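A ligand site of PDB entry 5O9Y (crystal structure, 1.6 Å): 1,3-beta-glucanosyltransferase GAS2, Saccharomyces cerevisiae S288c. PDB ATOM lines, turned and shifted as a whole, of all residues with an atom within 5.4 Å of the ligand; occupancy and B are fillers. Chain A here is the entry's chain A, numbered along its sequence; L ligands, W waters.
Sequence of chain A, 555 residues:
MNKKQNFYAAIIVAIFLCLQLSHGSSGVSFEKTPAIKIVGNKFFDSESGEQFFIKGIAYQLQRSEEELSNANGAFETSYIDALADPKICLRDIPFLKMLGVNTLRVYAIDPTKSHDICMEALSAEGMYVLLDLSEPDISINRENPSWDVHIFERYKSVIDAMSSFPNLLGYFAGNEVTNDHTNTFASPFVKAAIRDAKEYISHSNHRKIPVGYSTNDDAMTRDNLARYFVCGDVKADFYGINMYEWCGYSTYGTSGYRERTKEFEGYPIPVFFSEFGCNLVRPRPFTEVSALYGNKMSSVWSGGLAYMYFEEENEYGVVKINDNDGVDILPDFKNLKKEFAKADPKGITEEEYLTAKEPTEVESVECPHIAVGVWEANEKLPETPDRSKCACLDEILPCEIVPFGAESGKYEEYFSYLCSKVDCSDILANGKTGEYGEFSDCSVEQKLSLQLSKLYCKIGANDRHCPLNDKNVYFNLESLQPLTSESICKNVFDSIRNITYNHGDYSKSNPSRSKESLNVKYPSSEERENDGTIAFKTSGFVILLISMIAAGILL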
ATOM      1  N   GLN A  60     -33.912 -18.364  11.347  1.00  0.00           N
ATOM      2  CA  GLN A  60     -32.639 -18.530  10.641  1.00  0.00           C
ATOM      3  C   GLN A  60     -32.802 -19.589   9.558  1.00  0.00           C
ATOM      4  O   GLN A  60     -33.263 -20.699   9.821  1.00  0.00           O
ATOM      5  CB  GLN A  60     -31.526 -18.969  11.607  1.00  0.00           C
ATOM      6  CG  GLN A  60     -30.129 -18.942  11.008  1.00  0.00           C
ATOM      7  CD  GLN A  60     -29.618 -17.535  10.757  1.00  0.00           C
ATOM      8  OE1 GLN A  60     -29.614 -16.708  11.659  1.00  0.00           O
ATOM      9  NE2 GLN A  60     -29.178 -17.257   9.537  1.00  0.00           N
ATOM     10  N   GLN A  62     -31.102 -21.908   6.367  1.00  0.00           N
ATOM     11  CA  GLN A  62     -29.870 -22.552   5.903  1.00  0.00           C
ATOM     12  C   GLN A  62     -29.909 -22.806   4.402  1.00  0.00           C
ATOM     13  O   GLN A  62     -30.967 -22.717   3.772  1.00  0.00           O
ATOM     14  CB  GLN A  62     -29.654 -23.895   6.603  1.00  0.00           C
ATOM     15  CG  GLN A  62     -29.541 -23.841   8.120  1.00  0.00           C
ATOM     16  CD  GLN A  62     -28.395 -22.977   8.614  1.00  0.00           C
ATOM     17  OE1 GLN A  62     -28.516 -22.304   9.647  1.00  0.00           O
ATOM     18  NE2 GLN A  62     -27.273 -22.980   7.904  1.00  0.00           N
ATOM     19  N   TYR A 107     -29.026 -16.259  14.302  1.00  0.00           N
ATOM     20  CA  TYR A 107     -27.666 -16.791  14.518  1.00  0.00           C
ATOM     21  C   TYR A 107     -26.607 -16.166  13.616  1.00  0.00           C
ATOM     22  O   TYR A 107     -25.423 -16.209  13.955  1.00  0.00           O
ATOM     23  CB  TYR A 107     -27.659 -18.310  14.332  1.00  0.00           C
ATOM     24  CG  TYR A 107     -28.520 -19.045  15.335  1.00  0.00           C
ATOM     25  CD1 TYR A 107     -29.882 -19.216  15.115  1.00  0.00           C
ATOM     26  CD2 TYR A 107     -27.973 -19.569  16.502  1.00  0.00           C
ATOM     27  CE1 TYR A 107     -30.673 -19.886  16.025  1.00  0.00           C
ATOM     28  CE2 TYR A 107     -28.760 -20.243  17.420  1.00  0.00           C
ATOM     29  CZ  TYR A 107     -30.113 -20.393  17.181  1.00  0.00           C
ATOM     30  OH  TYR A 107     -30.897 -21.067  18.085  1.00  0.00           O
ATOM     31  N   ALA A 108     -27.015 -15.601  12.480  1.00  0.00           N
ATOM     32  CA  ALA A 108     -26.047 -15.002  11.565  1.00  0.00           C
ATOM     33  C   ALA A 108     -26.677 -13.957  10.657  1.00  0.00           C
ATOM     34  O   ALA A 108     -27.728 -14.206  10.063  1.00  0.00           O
ATOM     35  CB  ALA A 108     -25.373 -16.081  10.724  1.00  0.00           C
ATOM     36  N   ASP A 132     -26.567 -13.465  17.510  1.00  0.00           N
ATOM     37  CA  ASP A 132     -25.190 -13.952  17.665  1.00  0.00           C
ATOM     38  C   ASP A 132     -24.247 -13.080  16.840  1.00  0.00           C
ATOM     39  O   ASP A 132     -24.596 -12.649  15.744  1.00  0.00           O
ATOM     40  CB  ASP A 132     -25.069 -15.413  17.236  1.00  0.00           C
ATOM     41  CG  ASP A 132     -25.857 -16.353  18.131  1.00  0.00           C
ATOM     42  OD1 ASP A 132     -27.104 -16.373  18.017  1.00  0.00           O
ATOM     43  OD2 ASP A 132     -25.242 -17.081  18.936  1.00  0.00           O
ATOM     44  N   SER A 134     -21.116 -14.152  16.024  1.00  0.00           N
ATOM     45  CA  SER A 134     -20.316 -15.092  15.239  1.00  0.00           C
ATOM     46  C   SER A 134     -21.112 -15.727  14.114  1.00  0.00           C
ATOM     47  O   SER A 134     -22.327 -15.533  14.008  1.00  0.00           O
ATOM     48  CB  SER A 134     -19.775 -16.179  16.164  1.00  0.00           C
ATOM     49  OG  SER A 134     -20.837 -16.913  16.761  1.00  0.00           O
ATOM     50  N   GLU A 135     -20.412 -16.482  13.272  1.00  0.00           N
ATOM     51  CA  GLU A 135     -21.015 -17.277  12.203  1.00  0.00           C
ATOM     52  C   GLU A 135     -20.153 -18.535  12.010  1.00  0.00           C
ATOM     53  O   GLU A 135     -19.010 -18.559  12.478  1.00  0.00           O
ATOM     54  CB  GLU A 135     -21.142 -16.438  10.919  1.00  0.00           C
ATOM     55  CG  GLU A 135     -19.824 -15.908  10.349  1.00  0.00           C
ATOM     56  CD  GLU A 135     -19.356 -16.644   9.102  1.00  0.00           C
ATOM     57  OE1 GLU A 135     -19.651 -17.841   8.931  1.00  0.00           O
ATOM     58  OE2 GLU A 135     -18.648 -16.007   8.283  1.00  0.00           O
ATOM     59  N   PRO A 136     -20.681 -19.584  11.347  1.00  0.00           N
ATOM     60  CA  PRO A 136     -19.984 -20.883  11.321  1.00  0.00           C
ATOM     61  C   PRO A 136     -18.497 -20.853  10.909  1.00  0.00           C
ATOM     62  O   PRO A 136     -17.697 -21.601  11.472  1.00  0.00           O
ATOM     63  CB  PRO A 136     -20.807 -21.707  10.319  1.00  0.00           C
ATOM     64  CG  PRO A 136     -22.174 -21.132  10.420  1.00  0.00           C
ATOM     65  CD  PRO A 136     -21.951 -19.656  10.598  1.00  0.00           C
ATOM     66  N   ASP A 137     -18.156 -19.998   9.945  1.00  0.00           N
ATOM     67  CA  ASP A 137     -16.786 -19.841   9.457  1.00  0.00           C
ATOM     68  C   ASP A 137     -15.933 -18.801  10.213  1.00  0.00           C
ATOM     69  O   ASP A 137     -14.725 -18.749  10.007  1.00  0.00           O
ATOM     70  CB  ASP A 137     -16.781 -19.499   7.961  1.00  0.00           C
ATOM     71  CG  ASP A 137     -17.409 -20.601   7.094  1.00  0.00           C
ATOM     72  OD1 ASP A 137     -17.526 -21.757   7.556  1.00  0.00           O
ATOM     73  OD2 ASP A 137     -17.768 -20.298   5.946  1.00  0.00           O
ATOM     74  N   SER A 139     -15.897 -18.071  14.097  1.00  0.00           N
ATOM     75  CA  SER A 139     -16.274 -18.282  15.497  1.00  0.00           C
ATOM     76  C   SER A 139     -15.025 -18.660  16.283  1.00  0.00           C
ATOM     77  O   SER A 139     -13.992 -19.003  15.698  1.00  0.00           O
ATOM     78  CB  SER A 139     -17.263 -19.441  15.616  1.00  0.00           C
ATOM     79  OG  SER A 139     -18.503 -19.151  15.005  1.00  0.00           O
ATOM     80  N   ILE A 140     -15.129 -18.614  17.607  1.00  0.00           N
ATOM     81  CA  ILE A 140     -14.089 -19.160  18.477  1.00  0.00           C
ATOM     82  C   ILE A 140     -14.174 -20.675  18.329  1.00  0.00           C
ATOM     83  O   ILE A 140     -15.189 -21.286  18.676  1.00  0.00           O
ATOM     84  CB  ILE A 140     -14.280 -18.728  19.950  1.00  0.00           C
ATOM     85  CG1 ILE A 140     -14.113 -17.199  20.073  1.00  0.00           C
ATOM     86  CG2 ILE A 140     -13.277 -19.444  20.848  1.00  0.00           C
ATOM     87  CD1 ILE A 140     -14.662 -16.620  21.352  1.00  0.00           C
ATOM     88  N   ASN A 141     -13.112 -21.278  17.792  1.00  0.00           N
ATOM     89  CA  ASN A 141     -13.074 -22.710  17.520  1.00  0.00           C
ATOM     90  C   ASN A 141     -12.848 -23.469  18.811  1.00  0.00           C
ATOM     91  O   ASN A 141     -11.786 -23.379  19.399  1.00  0.00           O
ATOM     92  CB  ASN A 141     -11.978 -23.032  16.506  1.00  0.00           C
ATOM     93  CG  ASN A 141     -12.144 -24.411  15.878  1.00  0.00           C
ATOM     94  OD1 ASN A 141     -12.430 -25.391  16.571  1.00  0.00           O
ATOM     95  ND2 ASN A 141     -11.974 -24.498  14.561  1.00  0.00           N
ATOM     96  N   ARG A 142     -13.844 -24.246  19.255  1.00  0.00           N
ATOM     97  CA  ARG A 142     -13.710 -24.991  20.505  1.00  0.00           C
ATOM     98  C   ARG A 142     -12.590 -26.052  20.486  1.00  0.00           C
ATOM     99  O   ARG A 142     -12.084 -26.420  21.551  1.00  0.00           O
ATOM    100  CB  ARG A 142     -15.053 -25.614  20.925  1.00  0.00           C
ATOM    101  CG  ARG A 142     -15.555 -26.769  20.064  1.00  0.00           C
ATOM    102  CD  ARG A 142     -16.812 -27.397  20.654  1.00  0.00           C
ATOM    103  NE  ARG A 142     -18.016 -26.568  20.503  1.00  0.00           N
ATOM    104  CZ  ARG A 142     -18.774 -26.489  19.403  1.00  0.00           C
ATOM    105  NH1 ARG A 142     -18.475 -27.177  18.293  1.00  0.00           N
ATOM    106  NH2 ARG A 142     -19.855 -25.709  19.408  1.00  0.00           N
ATOM    107  N   GLU A 143     -12.221 -26.523  19.290  1.00  0.00           N
ATOM    108  CA  GLU A 143     -11.125 -27.501  19.114  1.00  0.00           C
ATOM    109  C   GLU A 143      -9.725 -26.851  19.105  1.00  0.00           C
ATOM    110  O   GLU A 143      -8.727 -27.544  19.343  1.00  0.00           O
ATOM    111  CB  GLU A 143     -11.314 -28.277  17.795  1.00  0.00           C
ATOM    112  CG  GLU A 143     -12.673 -28.935  17.596  1.00  0.00           C
ATOM    113  CD  GLU A 143     -13.018 -29.944  18.674  1.00  0.00           C
ATOM    114  OE1 GLU A 143     -12.095 -30.577  19.236  1.00  0.00           O
ATOM    115  OE2 GLU A 143     -14.226 -30.125  18.966  1.00  0.00           O
ATOM    116  N   ASN A 175     -21.746 -19.247  21.250  1.00  0.00           N
ATOM    117  CA  ASN A 175     -22.811 -20.243  21.374  1.00  0.00           C
ATOM    118  C   ASN A 175     -22.207 -21.624  21.580  1.00  0.00           C
ATOM    119  O   ASN A 175     -21.585 -22.167  20.658  1.00  0.00           O
ATOM    120  CB  ASN A 175     -23.705 -20.240  20.128  1.00  0.00           C
ATOM    121  CG  ASN A 175     -24.867 -21.214  20.253  1.00  0.00           C
ATOM    122  OD1 ASN A 175     -25.691 -21.076  21.159  1.00  0.00           O
ATOM    123  ND2 ASN A 175     -24.932 -22.195  19.373  1.00  0.00           N
ATOM    124  N   GLU A 176     -22.370 -22.183  22.780  1.00  0.00           N
ATOM    125  CA  GLU A 176     -21.937 -23.544  23.087  1.00  0.00           C
ATOM    126  C   GLU A 176     -20.482 -23.778  22.681  1.00  0.00           C
ATOM    127  O   GLU A 176     -20.173 -24.767  22.013  1.00  0.00           O
ATOM    128  CB  GLU A 176     -22.839 -24.563  22.392  1.00  0.00           C
ATOM    129  CG  GLU A 176     -24.325 -24.361  22.654  1.00  0.00           C
ATOM    130  CD  GLU A 176     -25.177 -25.506  22.144  1.00  0.00           C
ATOM    131  OE1 GLU A 176     -24.733 -26.276  21.261  1.00  0.00           O
ATOM    132  OE2 GLU A 176     -26.316 -25.628  22.646  1.00  0.00           O
ATOM    133  N   VAL A 177     -19.602 -22.858  23.073  1.00  0.00           N
ATOM    134  CA  VAL A 177     -18.189 -22.938  22.673  1.00  0.00           C
ATOM    135  C   VAL A 177     -17.586 -24.113  23.452  1.00  0.00           C
ATOM    136  O   VAL A 177     -17.354 -25.176  22.890  1.00  0.00           O
ATOM    137  CB  VAL A 177     -17.441 -21.603  22.850  1.00  0.00           C
ATOM    138  CG1 VAL A 177     -16.006 -21.720  22.361  1.00  0.00           C
ATOM    139  CG2 VAL A 177     -18.168 -20.484  22.087  1.00  0.00           C
ATOM    140  N   TYR A 244     -33.365 -28.400  26.554  1.00  0.00           N
ATOM    141  CA  TYR A 244     -34.199 -29.447  25.933  1.00  0.00           C
ATOM    142  C   TYR A 244     -34.609 -30.567  26.910  1.00  0.00           C
ATOM    143  O   TYR A 244     -34.955 -31.664  26.482  1.00  0.00           O
ATOM    144  CB  TYR A 244     -33.459 -30.022  24.724  1.00  0.00           C
ATOM    145  CG  TYR A 244     -33.285 -29.032  23.594  1.00  0.00           C
ATOM    146  CD1 TYR A 244     -34.248 -28.904  22.602  1.00  0.00           C
ATOM    147  CD2 TYR A 244     -32.155 -28.211  23.527  1.00  0.00           C
ATOM    148  CE1 TYR A 244     -34.108 -27.988  21.565  1.00  0.00           C
ATOM    149  CE2 TYR A 244     -31.994 -27.298  22.502  1.00  0.00           C
ATOM    150  CZ  TYR A 244     -32.970 -27.187  21.521  1.00  0.00           C
ATOM    151  OH  TYR A 244     -32.831 -26.284  20.491  1.00  0.00           O
ATOM    152  N   GLU A 275     -32.734 -21.426  23.667  1.00  0.00           N
ATOM    153  CA  GLU A 275     -33.471 -22.387  22.850  1.00  0.00           C
ATOM    154  C   GLU A 275     -34.318 -23.269  23.754  1.00  0.00           C
ATOM    155  O   GLU A 275     -33.924 -23.578  24.881  1.00  0.00           O
ATOM    156  CB  GLU A 275     -32.518 -23.289  22.063  1.00  0.00           C
ATOM    157  CG  GLU A 275     -31.760 -22.603  20.922  1.00  0.00           C
ATOM    158  CD  GLU A 275     -30.699 -23.501  20.311  1.00  0.00           C
ATOM    159  OE1 GLU A 275     -30.693 -24.717  20.582  1.00  0.00           O
ATOM    160  OE2 GLU A 275     -29.862 -22.974  19.556  1.00  0.00           O
ATOM    161  N   TYR A 307     -37.157 -23.314  19.489  1.00  0.00           N
ATOM    162  CA  TYR A 307     -36.350 -23.677  18.318  1.00  0.00           C
ATOM    163  C   TYR A 307     -37.170 -24.639  17.447  1.00  0.00           C
ATOM    164  O   TYR A 307     -37.433 -25.751  17.884  1.00  0.00           O
ATOM    165  CB  TYR A 307     -35.028 -24.332  18.743  1.00  0.00           C
ATOM    166  CG  TYR A 307     -34.121 -24.566  17.566  1.00  0.00           C
ATOM    167  CD1 TYR A 307     -34.213 -25.736  16.809  1.00  0.00           C
ATOM    168  CD2 TYR A 307     -33.191 -23.604  17.180  1.00  0.00           C
ATOM    169  CE1 TYR A 307     -33.395 -25.937  15.707  1.00  0.00           C
ATOM    170  CE2 TYR A 307     -32.364 -23.801  16.086  1.00  0.00           C
ATOM    171  CZ  TYR A 307     -32.471 -24.976  15.349  1.00  0.00           C
ATOM    172  OH  TYR A 307     -31.657 -25.178  14.259  1.00  0.00           O
ATOM    173  N   MET A 308     -37.606 -24.247  16.245  1.00  0.00           N
ATOM    174  CA  MET A 308     -37.455 -22.906  15.654  1.00  0.00           C
ATOM    175  C   MET A 308     -38.597 -22.645  14.659  1.00  0.00           C
ATOM    176  O   MET A 308     -39.499 -23.471  14.530  1.00  0.00           O
ATOM    177  CB  MET A 308     -36.091 -22.776  14.962  1.00  0.00           C
ATOM    178  CG  MET A 308     -35.936 -23.535  13.639  1.00  0.00           C
ATOM    179  SD  MET A 308     -34.779 -22.792  12.470  1.00  0.00           S
ATOM    180  CE  MET A 308     -35.372 -21.115  12.369  1.00  0.00           C
ATOM    181  N   GLU A 312     -36.345 -27.710   8.559  1.00  0.00           N
ATOM    182  CA  GLU A 312     -35.168 -27.977   7.723  1.00  0.00           C
ATOM    183  C   GLU A 312     -34.723 -29.437   7.843  1.00  0.00           C
ATOM    184  O   GLU A 312     -33.592 -29.716   8.249  1.00  0.00           O
ATOM    185  CB  GLU A 312     -34.038 -27.029   8.105  1.00  0.00           C
ATOM    186  CG  GLU A 312     -34.352 -25.553   7.897  1.00  0.00           C
ATOM    187  CD  GLU A 312     -33.163 -24.663   8.184  1.00  0.00           C
ATOM    188  OE1 GLU A 312     -32.857 -23.781   7.349  1.00  0.00           O
ATOM    189  OE2 GLU A 312     -32.530 -24.848   9.241  1.00  0.00           O
ATOM    190  N   TYR A 316     -37.840 -29.684  13.696  1.00  0.00           N
ATOM    191  CA  TYR A 316     -37.836 -28.587  14.685  1.00  0.00           C
ATOM    192  C   TYR A 316     -38.626 -27.347  14.257  1.00  0.00           C
ATOM    193  O   TYR A 316     -38.788 -26.417  15.050  1.00  0.00           O
ATOM    194  CB  TYR A 316     -36.406 -28.193  15.044  1.00  0.00           C
ATOM    195  CG  TYR A 316     -35.730 -29.174  15.970  1.00  0.00           C
ATOM    196  CD1 TYR A 316     -36.102 -29.262  17.314  1.00  0.00           C
ATOM    197  CD2 TYR A 316     -34.717 -30.016  15.508  1.00  0.00           C
ATOM    198  CE1 TYR A 316     -35.489 -30.162  18.176  1.00  0.00           C
ATOM    199  CE2 TYR A 316     -34.095 -30.919  16.365  1.00  0.00           C
ATOM    200  CZ  TYR A 316     -34.483 -30.984  17.691  1.00  0.00           C
ATOM    201  OH  TYR A 316     -33.871 -31.880  18.531  1.00  0.00           O
HETATM  202  C1  LIG L   1     -22.019 -20.309  15.249  1.00  0.00           C
HETATM  203  C2  LIG L   1     -23.431 -20.083  15.788  1.00  0.00           C
HETATM  204  C3  LIG L   1     -23.867 -18.627  15.575  1.00  0.00           C
HETATM  205  C4  LIG L   1     -21.673 -21.796  15.312  1.00  0.00           C
HETATM  206  C5  LIG L   1     -31.864 -31.322  21.261  1.00  0.00           C
HETATM  207  C6  LIG L   1     -31.615 -31.934  22.486  1.00  0.00           C
HETATM  208  C7  LIG L   1     -30.372 -31.791  23.099  1.00  0.00           C
HETATM  209  C8  LIG L   1     -29.375 -31.028  22.489  1.00  0.00           C
HETATM  210  C9  LIG L   1     -29.606 -30.403  21.260  1.00  0.00           C
HETATM  211  N1  LIG L   1     -30.870 -30.543  20.635  1.00  0.00           N
HETATM  212  C10 LIG L   1     -31.224 -29.927  19.322  1.00  0.00           C
HETATM  213  C11 LIG L   1     -30.244 -28.869  18.868  1.00  0.00           C
HETATM  214  C12 LIG L   1     -31.027 -28.080  17.838  1.00  0.00           C
HETATM  215  C13 LIG L   1     -30.012 -27.182  17.109  1.00  0.00           C
HETATM  216  C14 LIG L   1     -29.888 -25.869  17.193  1.00  0.00           C
HETATM  217  N2  LIG L   1     -29.098 -27.629  16.258  1.00  0.00           N
HETATM  218  N3  LIG L   1     -28.466 -26.673  15.858  1.00  0.00           N
HETATM  219  N4  LIG L   1     -28.861 -25.601  16.376  1.00  0.00           N
HETATM  220  C15 LIG L   1     -28.309 -24.269  16.069  1.00  0.00           C
HETATM  221  C16 LIG L   1     -26.808 -24.270  15.732  1.00  0.00           C
HETATM  222  O1  LIG L   1     -26.048 -24.446  16.933  1.00  0.00           O
HETATM  223  O2  LIG L   1     -29.084 -23.914  14.909  1.00  0.00           O
HETATM  224  C17 LIG L   1     -28.770 -22.611  14.397  1.00  0.00           C
HETATM  225  C18 LIG L   1     -29.769 -22.212  13.303  1.00  0.00           C
HETATM  226  O3  LIG L   1     -30.232 -23.367  12.618  1.00  0.00           O
HETATM  227  C19 LIG L   1     -27.339 -22.639  13.878  1.00  0.00           C
HETATM  228  O4  LIG L   1     -26.968 -21.374  13.306  1.00  0.00           O
HETATM  229  C20 LIG L   1     -26.418 -22.944  15.056  1.00  0.00           C
HETATM  230  O5  LIG L   1     -25.092 -23.060  14.528  1.00  0.00           O
HETATM  231  C21 LIG L   1     -24.103 -22.306  15.226  1.00  0.00           C
HETATM  232  C22 LIG L   1     -22.747 -22.617  14.617  1.00  0.00           C
HETATM  233  O6  LIG L   1     -22.484 -24.031  14.770  1.00  0.00           O
HETATM  234  O7  LIG L   1     -24.367 -20.904  15.080  1.00  0.00           O
HETATM  235  O8  LIG L   1     -23.876 -18.326  14.177  1.00  0.00           O
HETATM  236  O9  LIG L   1     -21.069 -19.552  16.018  1.00  0.00           O
HETATM  237  O10 LIG L   1     -20.408 -21.999  14.655  1.00  0.00           O
HETATM  238  C23 LIG L   1     -19.526 -22.904  15.322  1.00  0.00           C
HETATM  239  O11 LIG L   1     -19.185 -22.368  16.608  1.00  0.00           O
HETATM  240  C24 LIG L   1     -18.365 -23.272  17.370  1.00  0.00           C
HETATM  241  C25 LIG L   1     -18.202 -22.681  18.777  1.00  0.00           C
HETATM  242  O12 LIG L   1     -17.838 -21.301  18.689  1.00  0.00           O
HETATM  243  C26 LIG L   1     -17.019 -23.446  16.658  1.00  0.00           C
HETATM  244  O13 LIG L   1     -16.241 -24.423  17.361  1.00  0.00           O
HETATM  245  C27 LIG L   1     -17.243 -23.927  15.225  1.00  0.00           C
HETATM  246  O14 LIG L   1     -16.010 -23.891  14.511  1.00  0.00           O
HETATM  247  C28 LIG L   1     -18.252 -23.042  14.493  1.00  0.00           C
HETATM  248  O15 LIG L   1     -18.538 -23.612  13.212  1.00  0.00           O
HETATM  249  O   HOH W   1     -20.878 -24.938  12.679  1.00  0.00           O
HETATM  250  O   HOH W   2     -15.439 -26.676  16.108  1.00  0.00           O
HETATM  251  O   HOH W   3     -31.377 -22.573  10.560  1.00  0.00           O
HETATM  252  O   HOH W   4     -27.113 -19.959  10.645  1.00  0.00           O
HETATM  253  O   HOH W   5     -24.416 -23.793  11.227  1.00  0.00           O
HETATM  254  O   HOH W   6     -19.829 -19.450  18.839  1.00  0.00           O
HETATM  255  O   HOH W   7     -27.192 -23.896  19.421  1.00  0.00           O
HETATM  256  O   HOH W   8     -24.790 -20.137  12.283  1.00  0.00           O
HETATM  257  O   HOH W   9     -15.241 -25.084  12.184  1.00  0.00           O
HETATM  258  O   HOH W  10     -22.566 -23.300  18.302  1.00  0.00           O
HETATM  259  O   HOH W  11     -28.994 -30.688  25.730  1.00  0.00           O
HETATM  260  O   HOH W  12     -27.264 -28.387  22.499  1.00  0.00           O
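The backbone carbonyl oxygen (O) of Tyr 107 lies within hydrogen-bond range of an oxygen (O8) of the ligand. The backbone carbonyl oxygen (O) of Ile 140 is in hydrogen-bond range of an oxygen (O12) of the ligand (2.6 Å). O8 of the ligand sits at hydrogen-bond distance from O of Ser 134. The side-chain hydroxyl of Ser 134 sits at hydrogen-bond distance from an oxygen (O9) of the ligand. An oxygen (O9) of the ligand lies within hydrogen-bond range of the side-chain hydroxyl (OG) of Ser 139. O of Pro 136 sits at hydrogen-bond distance from O15 of the ligand. OH of Tyr 307 is in hydrogen-bond range of O3 of the ligand (2.8 Å). O13 of the ligand sits at hydrogen-bond distance from N of Arg 142 (3.1 Å).
OH of Tyr 107 sits at hydrogen-bond distance from OE2 of Glu 275, at 2.6 Å. The backbone NH (N) of Tyr 107 lies within hydrogen-bond range of the side-chain amide oxygen (OE1) of Gln 60 (2.7 Å). OG of Ser 139 is in hydrogen-bond range of O of Glu 135 (2.6 Å). The guanidinium group (NH2) of Arg 142 sits at hydrogen-bond distance from the backbone carbonyl oxygen (O) of Glu 176. The backbone NH (N) of Met 308 lies within hydrogen-bond range of the backbone carbonyl oxygen (O) of Tyr 316 (2.7 Å). The side-chain carboxylate (OE1) of Glu 275 sits at hydrogen-bond distance from the side-chain hydroxyl (OH) of Tyr 244, 2.7 Å away. The backbone NH (N) of Gln 62 is in hydrogen-bond range of the side-chain carboxylate (OE1) of Glu 312 (2.7 Å). N of Glu 143 is in hydrogen-bond range of OD1 of Asn 141 (3.0 Å).
Gln 62 touches the ligand. CB of Asp 132 touches C3 of the ligand (3.8 Å). Glu 135 touches the ligand (CA to O8, 3.6 Å). Asn 141 touches the ligand (CA to O13, 3.6 Å). ND2 of Asn 175 touches O1 of the ligand, at 3.5 Å. Val 177 touches the ligand. Tyr 244 touches the ligand. Glu 275 touches the ligand (OE1 to C14, 3.7 Å). OH of Tyr 316 touches C10 of the ligand, at 3.4 Å.
Water W2 bridges an oxygen (O13) of the ligand (2.7 Å) and the side-chain amide oxygen of Asn 141 (3.3 Å). Water W6 lies within hydrogen-bond range of an oxygen (O12) of the ligand (2.7 Å), the backbone NH of Asn 175 (3.1 Å) and the side-chain hydroxyl of Ser 134 (3.4 Å). Water W7 lies within hydrogen-bond range of an oxygen (O1) of the ligand, the side-chain carboxylate (OE2) of Glu 275 and the side-chain amide nitrogen (ND2) of Asn 175. Water W4 lies within hydrogen-bond range of OE1 of Gln 62 (2.9 Å) and O4 of the ligand (3.0 Å).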
